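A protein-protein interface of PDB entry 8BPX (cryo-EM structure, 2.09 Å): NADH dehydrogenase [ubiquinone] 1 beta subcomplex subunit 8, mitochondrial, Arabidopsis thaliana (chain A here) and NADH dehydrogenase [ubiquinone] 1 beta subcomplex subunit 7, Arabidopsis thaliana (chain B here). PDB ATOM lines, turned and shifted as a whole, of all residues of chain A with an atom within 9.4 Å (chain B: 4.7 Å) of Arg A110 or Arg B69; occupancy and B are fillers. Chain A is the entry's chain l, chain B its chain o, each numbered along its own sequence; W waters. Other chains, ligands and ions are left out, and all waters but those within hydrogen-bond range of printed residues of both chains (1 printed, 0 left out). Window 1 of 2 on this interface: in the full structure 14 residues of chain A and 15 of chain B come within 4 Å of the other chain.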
ATOM      1  N   VAL A 105       1.839  20.340  30.717  1.00  0.00           N
ATOM      2  CA  VAL A 105       2.171  21.756  30.525  1.00  0.00           C
ATOM      3  C   VAL A 105       1.145  22.388  29.587  1.00  0.00           C
ATOM      4  O   VAL A 105       0.803  21.790  28.552  1.00  0.00           O
ATOM      5  CB  VAL A 105       3.602  21.904  29.985  1.00  0.00           C
ATOM      6  CG1 VAL A 105       3.826  21.005  28.787  1.00  0.00           C
ATOM      7  CG2 VAL A 105       3.908  23.352  29.643  1.00  0.00           C
ATOM      8  N   PRO A 106       0.604  23.560  29.910  1.00  0.00           N
ATOM      9  CA  PRO A 106      -0.496  24.138  29.123  1.00  0.00           C
ATOM     10  C   PRO A 106      -0.072  25.015  27.953  1.00  0.00           C
ATOM     11  O   PRO A 106      -0.919  25.739  27.425  1.00  0.00           O
ATOM     12  CB  PRO A 106      -1.224  24.976  30.177  1.00  0.00           C
ATOM     13  CG  PRO A 106      -0.107  25.487  31.013  1.00  0.00           C
ATOM     14  CD  PRO A 106       0.832  24.321  31.150  1.00  0.00           C
ATOM     15  N   PHE A 107       1.196  24.993  27.549  1.00  0.00           N
ATOM     16  CA  PHE A 107       1.653  25.726  26.380  1.00  0.00           C
ATOM     17  C   PHE A 107       2.709  24.906  25.658  1.00  0.00           C
ATOM     18  O   PHE A 107       3.384  24.067  26.257  1.00  0.00           O
ATOM     19  CB  PHE A 107       2.212  27.118  26.740  1.00  0.00           C
ATOM     20  CG  PHE A 107       3.099  27.125  27.952  1.00  0.00           C
ATOM     21  CD1 PHE A 107       4.424  26.724  27.866  1.00  0.00           C
ATOM     22  CD2 PHE A 107       2.609  27.534  29.178  1.00  0.00           C
ATOM     23  CE1 PHE A 107       5.236  26.733  28.982  1.00  0.00           C
ATOM     24  CE2 PHE A 107       3.419  27.542  30.295  1.00  0.00           C
ATOM     25  CZ  PHE A 107       4.732  27.140  30.194  1.00  0.00           C
ATOM     26  N   THR A 108       2.757  25.155  24.367  1.00  0.00           N
ATOM     27  CA  THR A 108       3.807  24.509  23.567  1.00  0.00           C
ATOM     28  C   THR A 108       5.129  25.154  23.964  1.00  0.00           C
ATOM     29  O   THR A 108       5.142  26.248  24.471  1.00  0.00           O
ATOM     30  CB  THR A 108       3.532  24.573  22.064  1.00  0.00           C
ATOM     31  OG1 THR A 108       3.495  25.940  21.675  1.00  0.00           O
ATOM     32  CG2 THR A 108       2.272  23.850  21.654  1.00  0.00           C
ATOM     33  N   PRO A 109       6.255  24.518  23.657  1.00  0.00           N
ATOM     34  CA  PRO A 109       7.540  25.157  23.922  1.00  0.00           C
ATOM     35  C   PRO A 109       7.765  26.392  23.035  1.00  0.00           C
ATOM     36  O   PRO A 109       7.240  26.420  21.941  1.00  0.00           O
ATOM     37  CB  PRO A 109       8.556  24.000  23.667  1.00  0.00           C
ATOM     38  CG  PRO A 109       7.735  22.760  23.557  1.00  0.00           C
ATOM     39  CD  PRO A 109       6.391  23.209  23.043  1.00  0.00           C
ATOM     40  N   ARG A 110       8.493  27.376  23.587  1.00  0.00           N
ATOM     41  CA  ARG A 110       8.811  28.623  22.846  1.00  0.00           C
ATOM     42  C   ARG A 110       9.656  28.287  21.629  1.00  0.00           C
ATOM     43  O   ARG A 110      10.407  27.287  21.669  1.00  0.00           O
ATOM     44  CB  ARG A 110       9.676  29.588  23.662  1.00  0.00           C
ATOM     45  CG  ARG A 110       8.998  30.231  24.860  1.00  0.00           C
ATOM     46  CD  ARG A 110       9.887  31.272  25.505  1.00  0.00           C
ATOM     47  NE  ARG A 110       9.191  32.056  26.516  1.00  0.00           N
ATOM     48  CZ  ARG A 110       9.686  33.136  27.107  1.00  0.00           C
ATOM     49  NH1 ARG A 110      10.888  33.580  26.784  1.00  0.00           N
ATOM     50  NH2 ARG A 110       8.972  33.781  28.010  1.00  0.00           N
ATOM     51  N   VAL A 111       9.578  29.137  20.614  1.00  0.00           N
ATOM     52  CA  VAL A 111      10.352  28.916  19.371  1.00  0.00           C
ATOM     53  C   VAL A 111      10.849  30.280  19.020  1.00  0.00           C
ATOM     54  O   VAL A 111      10.059  31.135  18.703  1.00  0.00           O
ATOM     55  CB  VAL A 111       9.596  28.194  18.237  1.00  0.00           C
ATOM     56  CG1 VAL A 111      10.426  28.160  16.969  1.00  0.00           C
ATOM     57  CG2 VAL A 111       9.161  26.802  18.640  1.00  0.00           C
ATOM     58  N   TYR A 112      12.145  30.409  19.112  1.00  0.00           N
ATOM     59  CA  TYR A 112      12.778  31.686  18.819  1.00  0.00           C
ATOM     60  C   TYR A 112      12.940  31.791  17.316  1.00  0.00           C
ATOM     61  O   TYR A 112      13.074  30.777  16.700  1.00  0.00           O
ATOM     62  CB  TYR A 112      14.077  31.817  19.634  1.00  0.00           C
ATOM     63  CG  TYR A 112      13.789  32.147  21.068  1.00  0.00           C
ATOM     64  CD1 TYR A 112      13.462  31.158  21.981  1.00  0.00           C
ATOM     65  CD2 TYR A 112      13.776  33.461  21.485  1.00  0.00           C
ATOM     66  CE1 TYR A 112      13.186  31.475  23.298  1.00  0.00           C
ATOM     67  CE2 TYR A 112      13.509  33.790  22.797  1.00  0.00           C
ATOM     68  CZ  TYR A 112      13.219  32.791  23.704  1.00  0.00           C
ATOM     69  OH  TYR A 112      12.946  33.126  24.988  1.00  0.00           O
ATOM     70  N   PRO A 113      13.024  33.005  16.767  1.00  0.00           N
ATOM     71  CA  PRO A 113      13.321  33.202  15.343  1.00  0.00           C
ATOM     72  C   PRO A 113      14.776  32.933  14.994  1.00  0.00           C
ATOM     73  O   PRO A 113      15.604  32.657  15.872  1.00  0.00           O
ATOM     74  CB  PRO A 113      12.959  34.675  15.115  1.00  0.00           C
ATOM     75  CG  PRO A 113      13.187  35.304  16.449  1.00  0.00           C
ATOM     76  CD  PRO A 113      12.744  34.280  17.451  1.00  0.00           C
ATOM     77  N   ASN A 116      16.041  29.296  15.858  1.00  0.00           N
ATOM     78  CA  ASN A 116      16.174  29.203  17.330  1.00  0.00           C
ATOM     79  C   ASN A 116      17.450  29.943  17.806  1.00  0.00           C
ATOM     80  O   ASN A 116      17.984  29.493  18.745  1.00  0.00           O
ATOM     81  CB  ASN A 116      15.834  27.787  17.815  1.00  0.00           C
ATOM     82  CG  ASN A 116      14.526  27.730  18.557  1.00  0.00           C
ATOM     83  OD1 ASN A 116      14.404  28.271  19.649  1.00  0.00           O
ATOM     84  ND2 ASN A 116      13.539  27.101  17.947  1.00  0.00           N
ATOM     85  N   LEU A 117      17.732  31.134  17.229  1.00  0.00           N
ATOM     86  CA  LEU A 117      18.907  31.918  17.610  1.00  0.00           C
ATOM     87  C   LEU A 117      20.175  31.070  17.591  1.00  0.00           C
ATOM     88  O   LEU A 117      20.944  31.029  18.552  1.00  0.00           O
ATOM     89  CB  LEU A 117      18.711  32.571  18.980  1.00  0.00           C
ATOM     90  CG  LEU A 117      17.494  33.471  19.191  1.00  0.00           C
ATOM     91  CD1 LEU A 117      17.302  33.755  20.667  1.00  0.00           C
ATOM     92  CD2 LEU A 117      17.646  34.761  18.405  1.00  0.00           C
ATOM     93  N   GLY B  25      17.256  35.767  25.579  1.00  0.00           N
ATOM     94  CA  GLY B  25      15.909  35.294  25.854  1.00  0.00           C
ATOM     95  C   GLY B  25      14.803  36.294  25.585  1.00  0.00           C
ATOM     96  O   GLY B  25      13.708  35.911  25.659  1.00  0.00           O
ATOM     97  N   LEU B  65       1.741  36.414  22.516  1.00  0.00           N
ATOM     98  CA  LEU B  65       2.609  35.279  22.201  1.00  0.00           C
ATOM     99  C   LEU B  65       2.275  34.073  23.079  1.00  0.00           C
ATOM    100  O   LEU B  65       2.096  32.943  22.586  1.00  0.00           O
ATOM    101  CB  LEU B  65       4.077  35.675  22.376  1.00  0.00           C
ATOM    102  CG  LEU B  65       4.836  36.289  21.197  1.00  0.00           C
ATOM    103  CD1 LEU B  65       6.337  36.100  21.363  1.00  0.00           C
ATOM    104  CD2 LEU B  65       4.372  35.703  19.874  1.00  0.00           C
ATOM    105  N   VAL B  66       2.169  34.307  24.388  1.00  0.00           N
ATOM    106  CA  VAL B  66       1.848  33.220  25.310  1.00  0.00           C
ATOM    107  C   VAL B  66       0.475  32.636  25.001  1.00  0.00           C
ATOM    108  O   VAL B  66       0.277  31.419  25.066  1.00  0.00           O
ATOM    109  CB  VAL B  66       1.945  33.697  26.770  1.00  0.00           C
ATOM    110  CG1 VAL B  66       1.708  32.540  27.712  1.00  0.00           C
ATOM    111  CG2 VAL B  66       3.307  34.295  27.034  1.00  0.00           C
ATOM    112  N   MET B  67      -0.494  33.489  24.674  1.00  0.00           N
ATOM    113  CA  MET B  67      -1.835  32.996  24.378  1.00  0.00           C
ATOM    114  C   MET B  67      -1.841  32.106  23.142  1.00  0.00           C
ATOM    115  O   MET B  67      -2.528  31.081  23.116  1.00  0.00           O
ATOM    116  CB  MET B  67      -2.804  34.162  24.210  1.00  0.00           C
ATOM    117  CG  MET B  67      -3.155  34.845  25.507  1.00  0.00           C
ATOM    118  SD  MET B  67      -3.597  33.666  26.793  1.00  0.00           S
ATOM    119  CE  MET B  67      -2.344  34.033  28.019  1.00  0.00           C
ATOM    120  N   GLU B  68      -1.089  32.481  22.105  1.00  0.00           N
ATOM    121  CA  GLU B  68      -1.023  31.629  20.921  1.00  0.00           C
ATOM    122  C   GLU B  68      -0.416  30.275  21.259  1.00  0.00           C
ATOM    123  O   GLU B  68      -0.896  29.237  20.789  1.00  0.00           O
ATOM    124  CB  GLU B  68      -0.228  32.301  19.802  1.00  0.00           C
ATOM    125  CG  GLU B  68      -0.695  33.693  19.451  1.00  0.00           C
ATOM    126  CD  GLU B  68       0.304  34.439  18.591  1.00  0.00           C
ATOM    127  OE1 GLU B  68       1.408  34.744  19.088  1.00  0.00           O
ATOM    128  OE2 GLU B  68      -0.015  34.720  17.417  1.00  0.00           O
ATOM    129  N   ARG B  69       0.639  30.191  22.031  1.00  0.00           N
ATOM    130  CA  ARG B  69       1.239  28.912  22.485  1.00  0.00           C
ATOM    131  C   ARG B  69       0.278  28.151  23.424  1.00  0.00           C
ATOM    132  O   ARG B  69       0.338  26.951  23.472  1.00  0.00           O
ATOM    133  CB  ARG B  69       2.647  29.264  22.998  1.00  0.00           C
ATOM    134  CG  ARG B  69       3.738  29.516  21.979  1.00  0.00           C
ATOM    135  CD  ARG B  69       4.973  30.041  22.691  1.00  0.00           C
ATOM    136  NE  ARG B  69       5.325  29.247  23.855  1.00  0.00           N
ATOM    137  CZ  ARG B  69       5.733  29.733  25.018  1.00  0.00           C
ATOM    138  NH1 ARG B  69       5.881  31.031  25.185  1.00  0.00           N
ATOM    139  NH2 ARG B  69       6.008  28.911  26.011  1.00  0.00           N
ATOM    140  N   MET B  70      -0.600  28.834  24.133  1.00  0.00           N
ATOM    141  CA  MET B  70      -1.613  28.133  24.920  1.00  0.00           C
ATOM    142  C   MET B  70      -2.688  27.512  24.029  1.00  0.00           C
ATOM    143  O   MET B  70      -3.103  26.370  24.256  1.00  0.00           O
ATOM    144  CB  MET B  70      -2.240  29.085  25.937  1.00  0.00           C
ATOM    145  CG  MET B  70      -1.289  29.544  27.025  1.00  0.00           C
ATOM    146  SD  MET B  70      -2.085  30.457  28.357  1.00  0.00           S
ATOM    147  CE  MET B  70      -2.902  29.138  29.241  1.00  0.00           C
ATOM    148  N   LEU B  71      -3.158  28.247  23.014  1.00  0.00           N
ATOM    149  CA  LEU B  71      -4.133  27.671  22.086  1.00  0.00           C
ATOM    150  C   LEU B  71      -3.534  26.519  21.290  1.00  0.00           C
ATOM    151  O   LEU B  71      -4.211  25.517  21.029  1.00  0.00           O
ATOM    152  CB  LEU B  71      -4.697  28.732  21.138  1.00  0.00           C
ATOM    153  CG  LEU B  71      -5.872  29.577  21.645  1.00  0.00           C
ATOM    154  CD1 LEU B  71      -5.438  30.940  22.154  1.00  0.00           C
ATOM    155  CD2 LEU B  71      -6.919  29.719  20.561  1.00  0.00           C
ATOM    156  N   ALA B  72      -2.267  26.641  20.891  1.00  0.00           N
ATOM    157  CA  ALA B  72      -1.608  25.542  20.197  1.00  0.00           C
ATOM    158  C   ALA B  72      -1.575  24.287  21.064  1.00  0.00           C
ATOM    159  O   ALA B  72      -1.879  23.182  20.595  1.00  0.00           O
ATOM    160  CB  ALA B  72      -0.197  25.956  19.791  1.00  0.00           C
ATOM    161  N   MET B  73      -1.216  24.439  22.344  1.00  0.00           N
ATOM    162  CA  MET B  73      -1.210  23.276  23.226  1.00  0.00           C
ATOM    163  C   MET B  73      -2.619  22.745  23.463  1.00  0.00           C
ATOM    164  O   MET B  73      -2.799  21.538  23.634  1.00  0.00           O
ATOM    165  CB  MET B  73      -0.535  23.612  24.554  1.00  0.00           C
ATOM    166  CG  MET B  73      -0.439  22.443  25.525  1.00  0.00           C
ATOM    167  SD  MET B  73       0.274  20.946  24.809  1.00  0.00           S
ATOM    168  CE  MET B  73       2.020  21.325  24.841  1.00  0.00           C
HETATM  169  O   HOH W   1       7.059  33.411  24.847  1.00  0.00           O
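The backbone carbonyl oxygen of Thr A108 is in hydrogen-bond range of the guanidinium group of Arg B69 (3.1 Å). O of Gly B25 sits at hydrogen-bond distance from OH of Tyr A112 (3.0 Å).
The side-chain amide oxygen (OD1) of Asn A116 is in hydrogen-bond range of the backbone NH (N) of Tyr A112. OH of Tyr A112 sits at hydrogen-bond distance from NH1 of Arg A110, 2.8 Å away.
Among the printed residues, merely in contact across the chains: Arg A110 with Arg B69, Phe A107 with Arg B69, Val A105 with Met B73, Phe A107 with Met B73, Pro A106 with Met B70, Pro A106 with Met B73, Thr A108 with Met B73, Thr A108 with Ala B72, Arg A110 with Gly B25 and Pro A109 with Arg B69.
Printed residues of chain B within 4 Å of Phe A107: Arg B69 (3.3 Å) and Met B73 (3.4 Å). Of the printed residues of chain B, Thr A108 touches Arg B69 (3.1 Å), Ala B72 (3.7 Å) and Met B73 (3.6 Å). Arg A110 touches just these residues of chain B: Gly B25 (3.8 Å) and Arg B69 (3.2 Å). Printed residues of chain A within 4 Å of Gly B25: Arg A110 and Tyr A112. Arg B69 touches just these residues of chain A: Phe A107 (3.3 Å), Thr A108 (3.1 Å), Pro A109 (3.8 Å) and Arg A110 (3.2 Å). Leu B71 touches none of the printed residues of chain A. Of chain A, only Thr A108 comes within 4 Å of Ala B72. Printed residues of chain A within 4 Å of Met B73: Val A105 (3.3 Å), Pro A106 (3.6 Å), Phe A107 (3.4 Å) and Thr A108 (3.6 Å). The nearest printed residue of chain B that does not touch Arg A110 is Val B66 (5.8 Å). The nearest residue of chain A that does not touch Arg B69 is Pro A106 (4.3 Å).
Hydrophobic or aromatic side chains of chain B within 4 Å of the printed part of chain A: Met B70, Ala B72 and Met B73. Along chain A the printed residues that touch a printed residue of chain B span positions 105 to 112. Among the printed residues, 12 pairs touch across the chains. Among the printed residues, no Asp or Glu carboxylate lies within 4 Å of a Lys or Arg side-chain nitrogen of the other chain.
Water W1 bridges NH1 of Arg B69 and NE of Arg A110.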
